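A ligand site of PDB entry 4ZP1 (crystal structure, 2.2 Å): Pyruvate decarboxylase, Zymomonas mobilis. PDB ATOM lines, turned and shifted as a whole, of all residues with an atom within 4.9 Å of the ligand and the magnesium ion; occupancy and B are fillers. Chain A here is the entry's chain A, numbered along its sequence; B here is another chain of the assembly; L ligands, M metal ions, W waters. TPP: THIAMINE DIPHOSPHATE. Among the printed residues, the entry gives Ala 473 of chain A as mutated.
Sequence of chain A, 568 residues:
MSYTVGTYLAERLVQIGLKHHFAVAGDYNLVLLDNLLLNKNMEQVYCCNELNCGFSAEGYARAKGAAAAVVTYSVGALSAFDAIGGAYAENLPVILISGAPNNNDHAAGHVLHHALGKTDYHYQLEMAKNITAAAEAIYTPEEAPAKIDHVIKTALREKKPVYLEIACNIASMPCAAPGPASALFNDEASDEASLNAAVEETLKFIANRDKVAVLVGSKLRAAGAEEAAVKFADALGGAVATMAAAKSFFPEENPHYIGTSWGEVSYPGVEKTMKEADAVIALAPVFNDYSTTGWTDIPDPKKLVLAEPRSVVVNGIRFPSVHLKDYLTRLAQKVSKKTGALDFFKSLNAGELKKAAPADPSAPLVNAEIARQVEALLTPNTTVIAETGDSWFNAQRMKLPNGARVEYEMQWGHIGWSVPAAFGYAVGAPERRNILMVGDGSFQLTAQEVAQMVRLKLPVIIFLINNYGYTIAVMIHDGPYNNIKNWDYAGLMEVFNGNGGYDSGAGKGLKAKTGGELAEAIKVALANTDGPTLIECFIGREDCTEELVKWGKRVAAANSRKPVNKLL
The backbone NH (N) of Asp 440 is in hydrogen-bond range of the backbone carbonyl oxygen (O) of Ile 465 (3.1 Å).
A ring nitrogen (NE2) of His 414 sits close to the backbone carbonyl oxygen (O) of Val 75 of chain B, 3.3 Å away.
ND2 of Asn 467 lies within hydrogen-bond range of OG1 of Thr 471, 3.1 Å away.
The side-chain carboxylate of Asp 440 is in hydrogen-bond range of the backbone NH of Tyr 468.
Water W3 lies within hydrogen-bond range of O of Ile 465, ND2 of Asn 467, O2B of the ligand and N of Asp 440.
Water W1 lies within hydrogen-bond range of the backbone NH of Gly 439 (2.8 Å), an oxygen (O1A) of the ligand (2.9 Å), the backbone carbonyl oxygen of Thr 388 (2.9 Å) and the side-chain hydroxyl of Ser 442 (3.2 Å).
N of Gly 441 touches the magnesium ion (3.7 Å).
Four residues have an atom within 4 Å of the magnesium ion: Asp 440, Gly 441, Asn 467 and Gly 469.
An oxygen (O1A) of the ligand lies close to the backbone carbonyl oxygen (O) of Gly 439 (3.4 Å).
Residues that only touch the ligand: His 414, Tyr 470, Ala 25 of chain B, His 114 of chain B, Val 75 of chain B, Asp 390, Gly 26 of chain B, Gly 389 and Leu 445.
Hydrophobic or aromatic side chains that line the ligand: His 414, Ile 415, Leu 445, Tyr 470, Ile 472, Val 75 of chain B and His 114 of chain B.
Of the 29 residues printed, 20 come within 4 Å of the ligand.
Along chain A the residues within 4 Å of the ligand span positions 389 to 472.
The magnesium ion is bound by O2A of the ligand (1.9 Å), OD1 of Asp 440 (2.0 Å), O of Gly 469 (2.2 Å), water W3 (2.3 Å), OD1 of Asn 467 (2.3 Å) and O3B of the ligand (2.3 Å).
The backbone NH (N) of Ile 415 is in hydrogen-bond range of a nitrogen (N3') of the ligand, at 3.1 Å.
O1B of the ligand is in hydrogen-bond range of N of Ile 472, at 2.9 Å.
OG of Ser 442 sits at hydrogen-bond distance from O1A of the ligand, at 2.6 Å.
The backbone NH of Ser 442 lies within hydrogen-bond range of an oxygen (O1A) of the ligand (2.6 Å).
OE2 of Glu 50 of chain B is in hydrogen-bond range of N1' of the ligand (2.7 Å).
O3B of the ligand sits close to N of Thr 471 (2.8 Å).
N of Gly 441 sits at hydrogen-bond distance from O1A of the ligand (3.3 Å).
O of Gly 413 sits at hydrogen-bond distance from N4' of the ligand (2.7 Å).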
ATOM      1  N   THR A 388      27.722   5.714  23.071  1.00  0.00           N
ATOM      2  CA  THR A 388      26.669   4.916  23.683  1.00  0.00           C
ATOM      3  C   THR A 388      25.347   5.684  23.722  1.00  0.00           C
ATOM      4  O   THR A 388      25.275   6.796  24.236  1.00  0.00           O
ATOM      5  CB  THR A 388      27.037   4.523  25.134  1.00  0.00           C
ATOM      6  OG1 THR A 388      28.209   3.684  25.127  1.00  0.00           O
ATOM      7  CG2 THR A 388      25.886   3.793  25.807  1.00  0.00           C
ATOM      8  N   GLY A 389      24.302   5.062  23.174  1.00  0.00           N
ATOM      9  CA  GLY A 389      23.012   5.700  23.019  1.00  0.00           C
ATOM     10  C   GLY A 389      22.454   5.284  21.672  1.00  0.00           C
ATOM     11  O   GLY A 389      23.007   4.366  21.037  1.00  0.00           O
ATOM     12  N   ASP A 390      21.399   5.945  21.204  1.00  0.00           N
ATOM     13  CA  ASP A 390      20.827   5.609  19.901  1.00  0.00           C
ATOM     14  C   ASP A 390      21.866   5.795  18.790  1.00  0.00           C
ATOM     15  O   ASP A 390      21.739   5.222  17.709  1.00  0.00           O
ATOM     16  CB  ASP A 390      19.595   6.438  19.593  1.00  0.00           C
ATOM     17  CG  ASP A 390      18.727   5.810  18.507  1.00  0.00           C
ATOM     18  OD1 ASP A 390      18.721   4.563  18.407  1.00  0.00           O
ATOM     19  OD2 ASP A 390      18.055   6.550  17.759  1.00  0.00           O
ATOM     20  N   GLY A 413      31.239   1.014  27.654  1.00  0.00           N
ATOM     21  CA  GLY A 413      29.960   1.700  27.563  1.00  0.00           C
ATOM     22  C   GLY A 413      29.839   2.932  28.452  1.00  0.00           C
ATOM     23  O   GLY A 413      28.785   3.156  29.041  1.00  0.00           O
ATOM     24  N   HIS A 414      30.907   3.715  28.525  1.00  0.00           N
ATOM     25  CA  HIS A 414      30.935   4.896  29.383  1.00  0.00           C
ATOM     26  C   HIS A 414      30.409   6.111  28.653  1.00  0.00           C
ATOM     27  O   HIS A 414      31.064   6.607  27.739  1.00  0.00           O
ATOM     28  CB  HIS A 414      32.370   5.148  29.866  1.00  0.00           C
ATOM     29  CG  HIS A 414      32.476   6.182  30.942  1.00  0.00           C
ATOM     30  ND1 HIS A 414      32.252   7.526  30.716  1.00  0.00           N
ATOM     31  CD2 HIS A 414      32.780   6.070  32.259  1.00  0.00           C
ATOM     32  CE1 HIS A 414      32.419   8.185  31.849  1.00  0.00           C
ATOM     33  NE2 HIS A 414      32.745   7.328  32.797  1.00  0.00           N
ATOM     34  N   ILE A 415      29.234   6.614  29.024  1.00  0.00           N
ATOM     35  CA  ILE A 415      28.725   7.785  28.320  1.00  0.00           C
ATOM     36  C   ILE A 415      29.697   8.940  28.525  1.00  0.00           C
ATOM     37  O   ILE A 415      30.289   9.080  29.606  1.00  0.00           O
ATOM     38  CB  ILE A 415      27.299   8.183  28.765  1.00  0.00           C
ATOM     39  CG1 ILE A 415      27.293   8.782  30.168  1.00  0.00           C
ATOM     40  CG2 ILE A 415      26.356   6.989  28.693  1.00  0.00           C
ATOM     41  CD1 ILE A 415      25.924   9.311  30.569  1.00  0.00           C
ATOM     42  N   GLY A 439      24.998  11.999  21.939  1.00  0.00           N
ATOM     43  CA  GLY A 439      23.739  12.470  22.482  1.00  0.00           C
ATOM     44  C   GLY A 439      23.948  13.555  23.518  1.00  0.00           C
ATOM     45  O   GLY A 439      25.035  13.681  24.075  1.00  0.00           O
ATOM     46  N   ASP A 440      22.898  14.334  23.781  1.00  0.00           N
ATOM     47  CA  ASP A 440      23.014  15.444  24.722  1.00  0.00           C
ATOM     48  C   ASP A 440      23.414  14.965  26.121  1.00  0.00           C
ATOM     49  O   ASP A 440      24.252  15.592  26.777  1.00  0.00           O
ATOM     50  CB  ASP A 440      21.693  16.234  24.793  1.00  0.00           C
ATOM     51  CG  ASP A 440      20.489  15.351  25.096  1.00  0.00           C
ATOM     52  OD1 ASP A 440      20.550  14.137  24.841  1.00  0.00           O
ATOM     53  OD2 ASP A 440      19.467  15.881  25.581  1.00  0.00           O
ATOM     54  N   GLY A 441      22.837  13.854  26.555  1.00  0.00           N
ATOM     55  CA  GLY A 441      23.118  13.314  27.871  1.00  0.00           C
ATOM     56  C   GLY A 441      24.589  12.988  28.086  1.00  0.00           C
ATOM     57  O   GLY A 441      25.168  13.365  29.104  1.00  0.00           O
ATOM     58  N   SER A 442      25.179  12.291  27.116  1.00  0.00           N
ATOM     59  CA  SER A 442      26.585  11.897  27.204  1.00  0.00           C
ATOM     60  C   SER A 442      27.505  13.093  27.085  1.00  0.00           C
ATOM     61  O   SER A 442      28.549  13.169  27.753  1.00  0.00           O
ATOM     62  CB  SER A 442      26.919  10.869  26.107  1.00  0.00           C
ATOM     63  OG  SER A 442      25.990   9.807  26.118  1.00  0.00           O
ATOM     64  N   PHE A 443      27.130  14.031  26.213  1.00  0.00           N
ATOM     65  CA  PHE A 443      27.961  15.188  25.917  1.00  0.00           C
ATOM     66  C   PHE A 443      28.230  16.028  27.184  1.00  0.00           C
ATOM     67  O   PHE A 443      29.288  16.648  27.292  1.00  0.00           O
ATOM     68  CB  PHE A 443      27.312  16.052  24.834  1.00  0.00           C
ATOM     69  CG  PHE A 443      28.126  17.264  24.416  1.00  0.00           C
ATOM     70  CD1 PHE A 443      29.078  17.172  23.416  1.00  0.00           C
ATOM     71  CD2 PHE A 443      27.925  18.496  25.029  1.00  0.00           C
ATOM     72  CE1 PHE A 443      29.820  18.283  23.032  1.00  0.00           C
ATOM     73  CE2 PHE A 443      28.662  19.614  24.651  1.00  0.00           C
ATOM     74  CZ  PHE A 443      29.606  19.510  23.655  1.00  0.00           C
ATOM     75  N   LEU A 445      28.855  15.089  30.187  1.00  0.00           N
ATOM     76  CA  LEU A 445      29.850  14.543  31.107  1.00  0.00           C
ATOM     77  C   LEU A 445      31.273  15.029  30.826  1.00  0.00           C
ATOM     78  O   LEU A 445      32.097  15.103  31.730  1.00  0.00           O
ATOM     79  CB  LEU A 445      29.847  13.013  31.072  1.00  0.00           C
ATOM     80  CG  LEU A 445      28.817  12.278  31.944  1.00  0.00           C
ATOM     81  CD1 LEU A 445      27.462  12.230  31.249  1.00  0.00           C
ATOM     82  CD2 LEU A 445      29.317  10.886  32.304  1.00  0.00           C
ATOM     83  N   ILE A 465      22.942  15.182  19.195  1.00  0.00           N
ATOM     84  CA  ILE A 465      21.524  14.826  19.149  1.00  0.00           C
ATOM     85  C   ILE A 465      20.788  15.339  20.386  1.00  0.00           C
ATOM     86  O   ILE A 465      20.834  14.707  21.442  1.00  0.00           O
ATOM     87  CB  ILE A 465      21.338  13.316  19.045  1.00  0.00           C
ATOM     88  CG1 ILE A 465      22.291  12.738  18.005  1.00  0.00           C
ATOM     89  CG2 ILE A 465      19.906  12.992  18.685  1.00  0.00           C
ATOM     90  CD1 ILE A 465      22.110  13.343  16.633  1.00  0.00           C
ATOM     91  N   ASN A 467      17.734  15.377  22.061  1.00  0.00           N
ATOM     92  CA  ASN A 467      16.406  14.808  22.242  1.00  0.00           C
ATOM     93  C   ASN A 467      15.907  15.046  23.666  1.00  0.00           C
ATOM     94  O   ASN A 467      14.873  14.514  24.064  1.00  0.00           O
ATOM     95  CB  ASN A 467      16.426  13.311  21.927  1.00  0.00           C
ATOM     96  CG  ASN A 467      17.475  12.560  22.729  1.00  0.00           C
ATOM     97  OD1 ASN A 467      17.955  13.060  23.752  1.00  0.00           O
ATOM     98  ND2 ASN A 467      17.845  11.368  22.266  1.00  0.00           N
ATOM     99  N   TYR A 468      16.680  15.822  24.433  1.00  0.00           N
ATOM    100  CA  TYR A 468      16.321  16.250  25.782  1.00  0.00           C
ATOM    101  C   TYR A 468      16.165  15.109  26.802  1.00  0.00           C
ATOM    102  O   TYR A 468      15.103  14.984  27.428  1.00  0.00           O
ATOM    103  CB  TYR A 468      15.038  17.092  25.718  1.00  0.00           C
ATOM    104  CG  TYR A 468      14.749  17.873  26.982  1.00  0.00           C
ATOM    105  CD1 TYR A 468      15.764  18.580  27.621  1.00  0.00           C
ATOM    106  CD2 TYR A 468      13.476  17.898  27.535  1.00  0.00           C
ATOM    107  CE1 TYR A 468      15.511  19.301  28.776  1.00  0.00           C
ATOM    108  CE2 TYR A 468      13.217  18.625  28.696  1.00  0.00           C
ATOM    109  CZ  TYR A 468      14.239  19.316  29.306  1.00  0.00           C
ATOM    110  OH  TYR A 468      13.999  20.036  30.457  1.00  0.00           O
ATOM    111  N   GLY A 469      17.199  14.299  26.977  1.00  0.00           N
ATOM    112  CA  GLY A 469      17.191  13.267  28.009  1.00  0.00           C
ATOM    113  C   GLY A 469      17.947  11.995  27.660  1.00  0.00           C
ATOM    114  O   GLY A 469      18.437  11.850  26.539  1.00  0.00           O
ATOM    115  N   TYR A 470      18.045  11.069  28.617  1.00  0.00           N
ATOM    116  CA  TYR A 470      18.684   9.759  28.402  1.00  0.00           C
ATOM    117  C   TYR A 470      17.740   8.778  27.679  1.00  0.00           C
ATOM    118  O   TYR A 470      17.149   7.899  28.324  1.00  0.00           O
ATOM    119  CB  TYR A 470      19.115   9.124  29.730  1.00  0.00           C
ATOM    120  CG  TYR A 470      20.109   9.896  30.572  1.00  0.00           C
ATOM    121  CD1 TYR A 470      21.005  10.791  30.005  1.00  0.00           C
ATOM    122  CD2 TYR A 470      20.154   9.714  31.955  1.00  0.00           C
ATOM    123  CE1 TYR A 470      21.916  11.485  30.796  1.00  0.00           C
ATOM    124  CE2 TYR A 470      21.058  10.403  32.743  1.00  0.00           C
ATOM    125  CZ  TYR A 470      21.935  11.295  32.163  1.00  0.00           C
ATOM    126  OH  TYR A 470      22.826  11.979  32.963  1.00  0.00           O
ATOM    127  N   THR A 471      17.606   8.911  26.363  1.00  0.00           N
ATOM    128  CA  THR A 471      16.580   8.177  25.624  1.00  0.00           C
ATOM    129  C   THR A 471      16.792   6.650  25.633  1.00  0.00           C
ATOM    130  O   THR A 471      15.828   5.892  25.748  1.00  0.00           O
ATOM    131  CB  THR A 471      16.487   8.664  24.164  1.00  0.00           C
ATOM    132  OG1 THR A 471      15.862   9.959  24.139  1.00  0.00           O
ATOM    133  CG2 THR A 471      15.654   7.705  23.320  1.00  0.00           C
ATOM    134  N   ILE A 472      18.042   6.212  25.502  1.00  0.00           N
ATOM    135  CA  ILE A 472      18.347   4.774  25.542  1.00  0.00           C
ATOM    136  C   ILE A 472      17.954   4.200  26.910  1.00  0.00           C
ATOM    137  O   ILE A 472      17.506   3.058  27.006  1.00  0.00           O
ATOM    138  CB  ILE A 472      19.831   4.478  25.251  1.00  0.00           C
ATOM    139  CG1 ILE A 472      20.148   2.998  25.479  1.00  0.00           C
ATOM    140  CG2 ILE A 472      20.721   5.349  26.117  1.00  0.00           C
ATOM    141  CD1 ILE A 472      21.504   2.572  24.930  1.00  0.00           C
ATOM    142  N   ALA A 473      18.124   5.003  27.953  1.00  0.00           N
ATOM    143  CA  ALA A 473      17.694   4.625  29.295  1.00  0.00           C
ATOM    144  C   ALA A 473      16.170   4.595  29.384  1.00  0.00           C
ATOM    145  O   ALA A 473      15.598   3.795  30.120  1.00  0.00           O
ATOM    146  CB  ALA A 473      18.281   5.563  30.337  1.00  0.00           C
ATOM    147  N   VAL B  24      23.531   9.454  39.631  1.00  0.00           N
ATOM    148  CA  VAL B  24      23.678   9.426  38.196  1.00  0.00           C
ATOM    149  C   VAL B  24      23.057   8.107  37.736  1.00  0.00           C
ATOM    150  O   VAL B  24      23.527   7.034  38.121  1.00  0.00           O
ATOM    151  CB  VAL B  24      25.151   9.518  37.745  1.00  0.00           C
ATOM    152  CG1 VAL B  24      25.278   9.316  36.245  1.00  0.00           C
ATOM    153  CG2 VAL B  24      25.758  10.858  38.172  1.00  0.00           C
ATOM    154  N   ALA B  25      21.990   8.191  36.956  1.00  0.00           N
ATOM    155  CA  ALA B  25      21.274   6.981  36.552  1.00  0.00           C
ATOM    156  C   ALA B  25      22.137   6.071  35.658  1.00  0.00           C
ATOM    157  O   ALA B  25      22.999   6.527  34.924  1.00  0.00           O
ATOM    158  CB  ALA B  25      19.981   7.340  35.846  1.00  0.00           C
ATOM    159  N   GLY B  26      21.881   4.768  35.754  1.00  0.00           N
ATOM    160  CA  GLY B  26      22.564   3.787  34.950  1.00  0.00           C
ATOM    161  C   GLY B  26      21.732   2.519  34.968  1.00  0.00           C
ATOM    162  O   GLY B  26      20.967   2.309  35.918  1.00  0.00           O
ATOM    163  N   ASP B  27      21.874   1.658  33.966  1.00  0.00           N
ATOM    164  CA  ASP B  27      20.980   0.513  33.874  1.00  0.00           C
ATOM    165  C   ASP B  27      21.199  -0.503  34.998  1.00  0.00           C
ATOM    166  O   ASP B  27      20.412  -1.424  35.168  1.00  0.00           O
ATOM    167  CB  ASP B  27      21.113  -0.174  32.506  1.00  0.00           C
ATOM    168  CG  ASP B  27      22.409  -0.963  32.361  1.00  0.00           C
ATOM    169  OD1 ASP B  27      23.392  -0.646  33.072  1.00  0.00           O
ATOM    170  OD2 ASP B  27      22.426  -1.894  31.534  1.00  0.00           O
ATOM    171  N   GLU B  50      29.862  11.310  37.383  1.00  0.00           N
ATOM    172  CA  GLU B  50      30.010  10.678  38.684  1.00  0.00           C
ATOM    173  C   GLU B  50      31.065  11.343  39.570  1.00  0.00           C
ATOM    174  O   GLU B  50      30.953  11.329  40.793  1.00  0.00           O
ATOM    175  CB  GLU B  50      30.345   9.198  38.525  1.00  0.00           C
ATOM    176  CG  GLU B  50      29.213   8.365  37.920  1.00  0.00           C
ATOM    177  CD  GLU B  50      29.095   8.531  36.419  1.00  0.00           C
ATOM    178  OE1 GLU B  50      29.971   9.182  35.807  1.00  0.00           O
ATOM    179  OE2 GLU B  50      28.120   7.992  35.835  1.00  0.00           O
ATOM    180  N   THR B  72      26.224   3.840  38.959  1.00  0.00           N
ATOM    181  CA  THR B  72      26.071   2.533  38.347  1.00  0.00           C
ATOM    182  C   THR B  72      27.404   1.784  38.348  1.00  0.00           C
ATOM    183  O   THR B  72      28.449   2.351  38.665  1.00  0.00           O
ATOM    184  CB  THR B  72      25.516   2.661  36.917  1.00  0.00           C
ATOM    185  OG1 THR B  72      25.052   1.381  36.463  1.00  0.00           O
ATOM    186  CG2 THR B  72      26.572   3.196  35.964  1.00  0.00           C
ATOM    187  N   VAL B  75      31.568   1.880  35.360  1.00  0.00           N
ATOM    188  CA  VAL B  75      31.743   3.108  34.608  1.00  0.00           C
ATOM    189  C   VAL B  75      31.403   4.313  35.473  1.00  0.00           C
ATOM    190  O   VAL B  75      31.987   5.377  35.328  1.00  0.00           O
ATOM    191  CB  VAL B  75      30.880   3.125  33.325  1.00  0.00           C
ATOM    192  CG1 VAL B  75      31.392   2.081  32.341  1.00  0.00           C
ATOM    193  CG2 VAL B  75      29.424   2.881  33.671  1.00  0.00           C
ATOM    194  N   GLY B  76      30.463   4.131  36.386  1.00  0.00           N
ATOM    195  CA  GLY B  76      30.096   5.196  37.296  1.00  0.00           C
ATOM    196  C   GLY B  76      31.004   5.220  38.513  1.00  0.00           C
ATOM    197  O   GLY B  76      31.621   6.241  38.828  1.00  0.00           O
ATOM    198  N   HIS B 114      29.897  -2.907  30.622  1.00  0.00           N
ATOM    199  CA  HIS B 114      30.372  -2.073  31.715  1.00  0.00           C
ATOM    200  C   HIS B 114      31.408  -2.765  32.597  1.00  0.00           C
ATOM    201  O   HIS B 114      31.709  -2.275  33.668  1.00  0.00           O
ATOM    202  CB  HIS B 114      29.227  -1.605  32.618  1.00  0.00           C
ATOM    203  CG  HIS B 114      28.280  -0.646  31.973  1.00  0.00           C
ATOM    204  ND1 HIS B 114      28.590   0.040  30.805  1.00  0.00           N
ATOM    205  CD2 HIS B 114      27.044  -0.228  32.321  1.00  0.00           C
ATOM    206  CE1 HIS B 114      27.581   0.811  30.474  1.00  0.00           C
ATOM    207  NE2 HIS B 114      26.625   0.666  31.368  1.00  0.00           N
HETATM  208  N1' TPP L   1      27.194   6.779  33.593  1.00  0.00           N
HETATM  209  C2' TPP L   1      28.291   6.423  32.819  1.00  0.00           C
HETATM  210  CM2 TPP L   1      29.645   6.993  33.150  1.00  0.00           C
HETATM  211  N3' TPP L   1      28.147   5.549  31.752  1.00  0.00           N
HETATM  212  C4' TPP L   1      26.903   5.020  31.450  1.00  0.00           C
HETATM  213  N4' TPP L   1      26.763   4.178  30.423  1.00  0.00           N
HETATM  214  C5' TPP L   1      25.790   5.366  32.218  1.00  0.00           C
HETATM  215  C6' TPP L   1      25.952   6.244  33.299  1.00  0.00           C
HETATM  216  C7' TPP L   1      24.417   4.807  31.927  1.00  0.00           C
HETATM  217  N3  TPP L   1      23.831   5.252  30.678  1.00  0.00           N
HETATM  218  C2  TPP L   1      23.825   4.506  29.509  1.00  0.00           C
HETATM  219  S1  TPP L   1      23.092   5.240  28.292  1.00  0.00           S
HETATM  220  C5  TPP L   1      22.755   6.531  29.176  1.00  0.00           C
HETATM  221  C4  TPP L   1      23.197   6.430  30.491  1.00  0.00           C
HETATM  222  CM4 TPP L   1      23.017   7.482  31.555  1.00  0.00           C
HETATM  223  C6  TPP L   1      21.998   7.636  28.461  1.00  0.00           C
HETATM  224  C7  TPP L   1      22.812   8.361  27.382  1.00  0.00           C
HETATM  225  O7  TPP L   1      22.252   9.646  27.140  1.00  0.00           O
HETATM  226  PA  TPP L   1      22.342  10.401  25.701  1.00  0.00           P
HETATM  227  O1A TPP L   1      23.748  10.877  25.415  1.00  0.00           O
HETATM  228  O2A TPP L   1      21.385  11.574  25.660  1.00  0.00           O
HETATM  229  O3A TPP L   1      21.929   9.234  24.660  1.00  0.00           O
HETATM  230  PB  TPP L   1      20.507   9.102  23.918  1.00  0.00           P
HETATM  231  O1B TPP L   1      20.036   7.669  24.062  1.00  0.00           O
HETATM  232  O2B TPP L   1      20.668   9.411  22.448  1.00  0.00           O
HETATM  233  O3B TPP L   1      19.478  10.036  24.534  1.00  0.00           O
HETATM  234 MG    MG M   1      19.835  12.316  24.926  1.00  0.00          MG
HETATM  235  O   HOH W   1      24.837   9.464  23.158  1.00  0.00           O
HETATM  236  O   HOH W   2      23.227   8.944  21.147  1.00  0.00           O
HETATM  237  O   HOH W   3      20.474  12.253  22.752  1.00  0.00           O
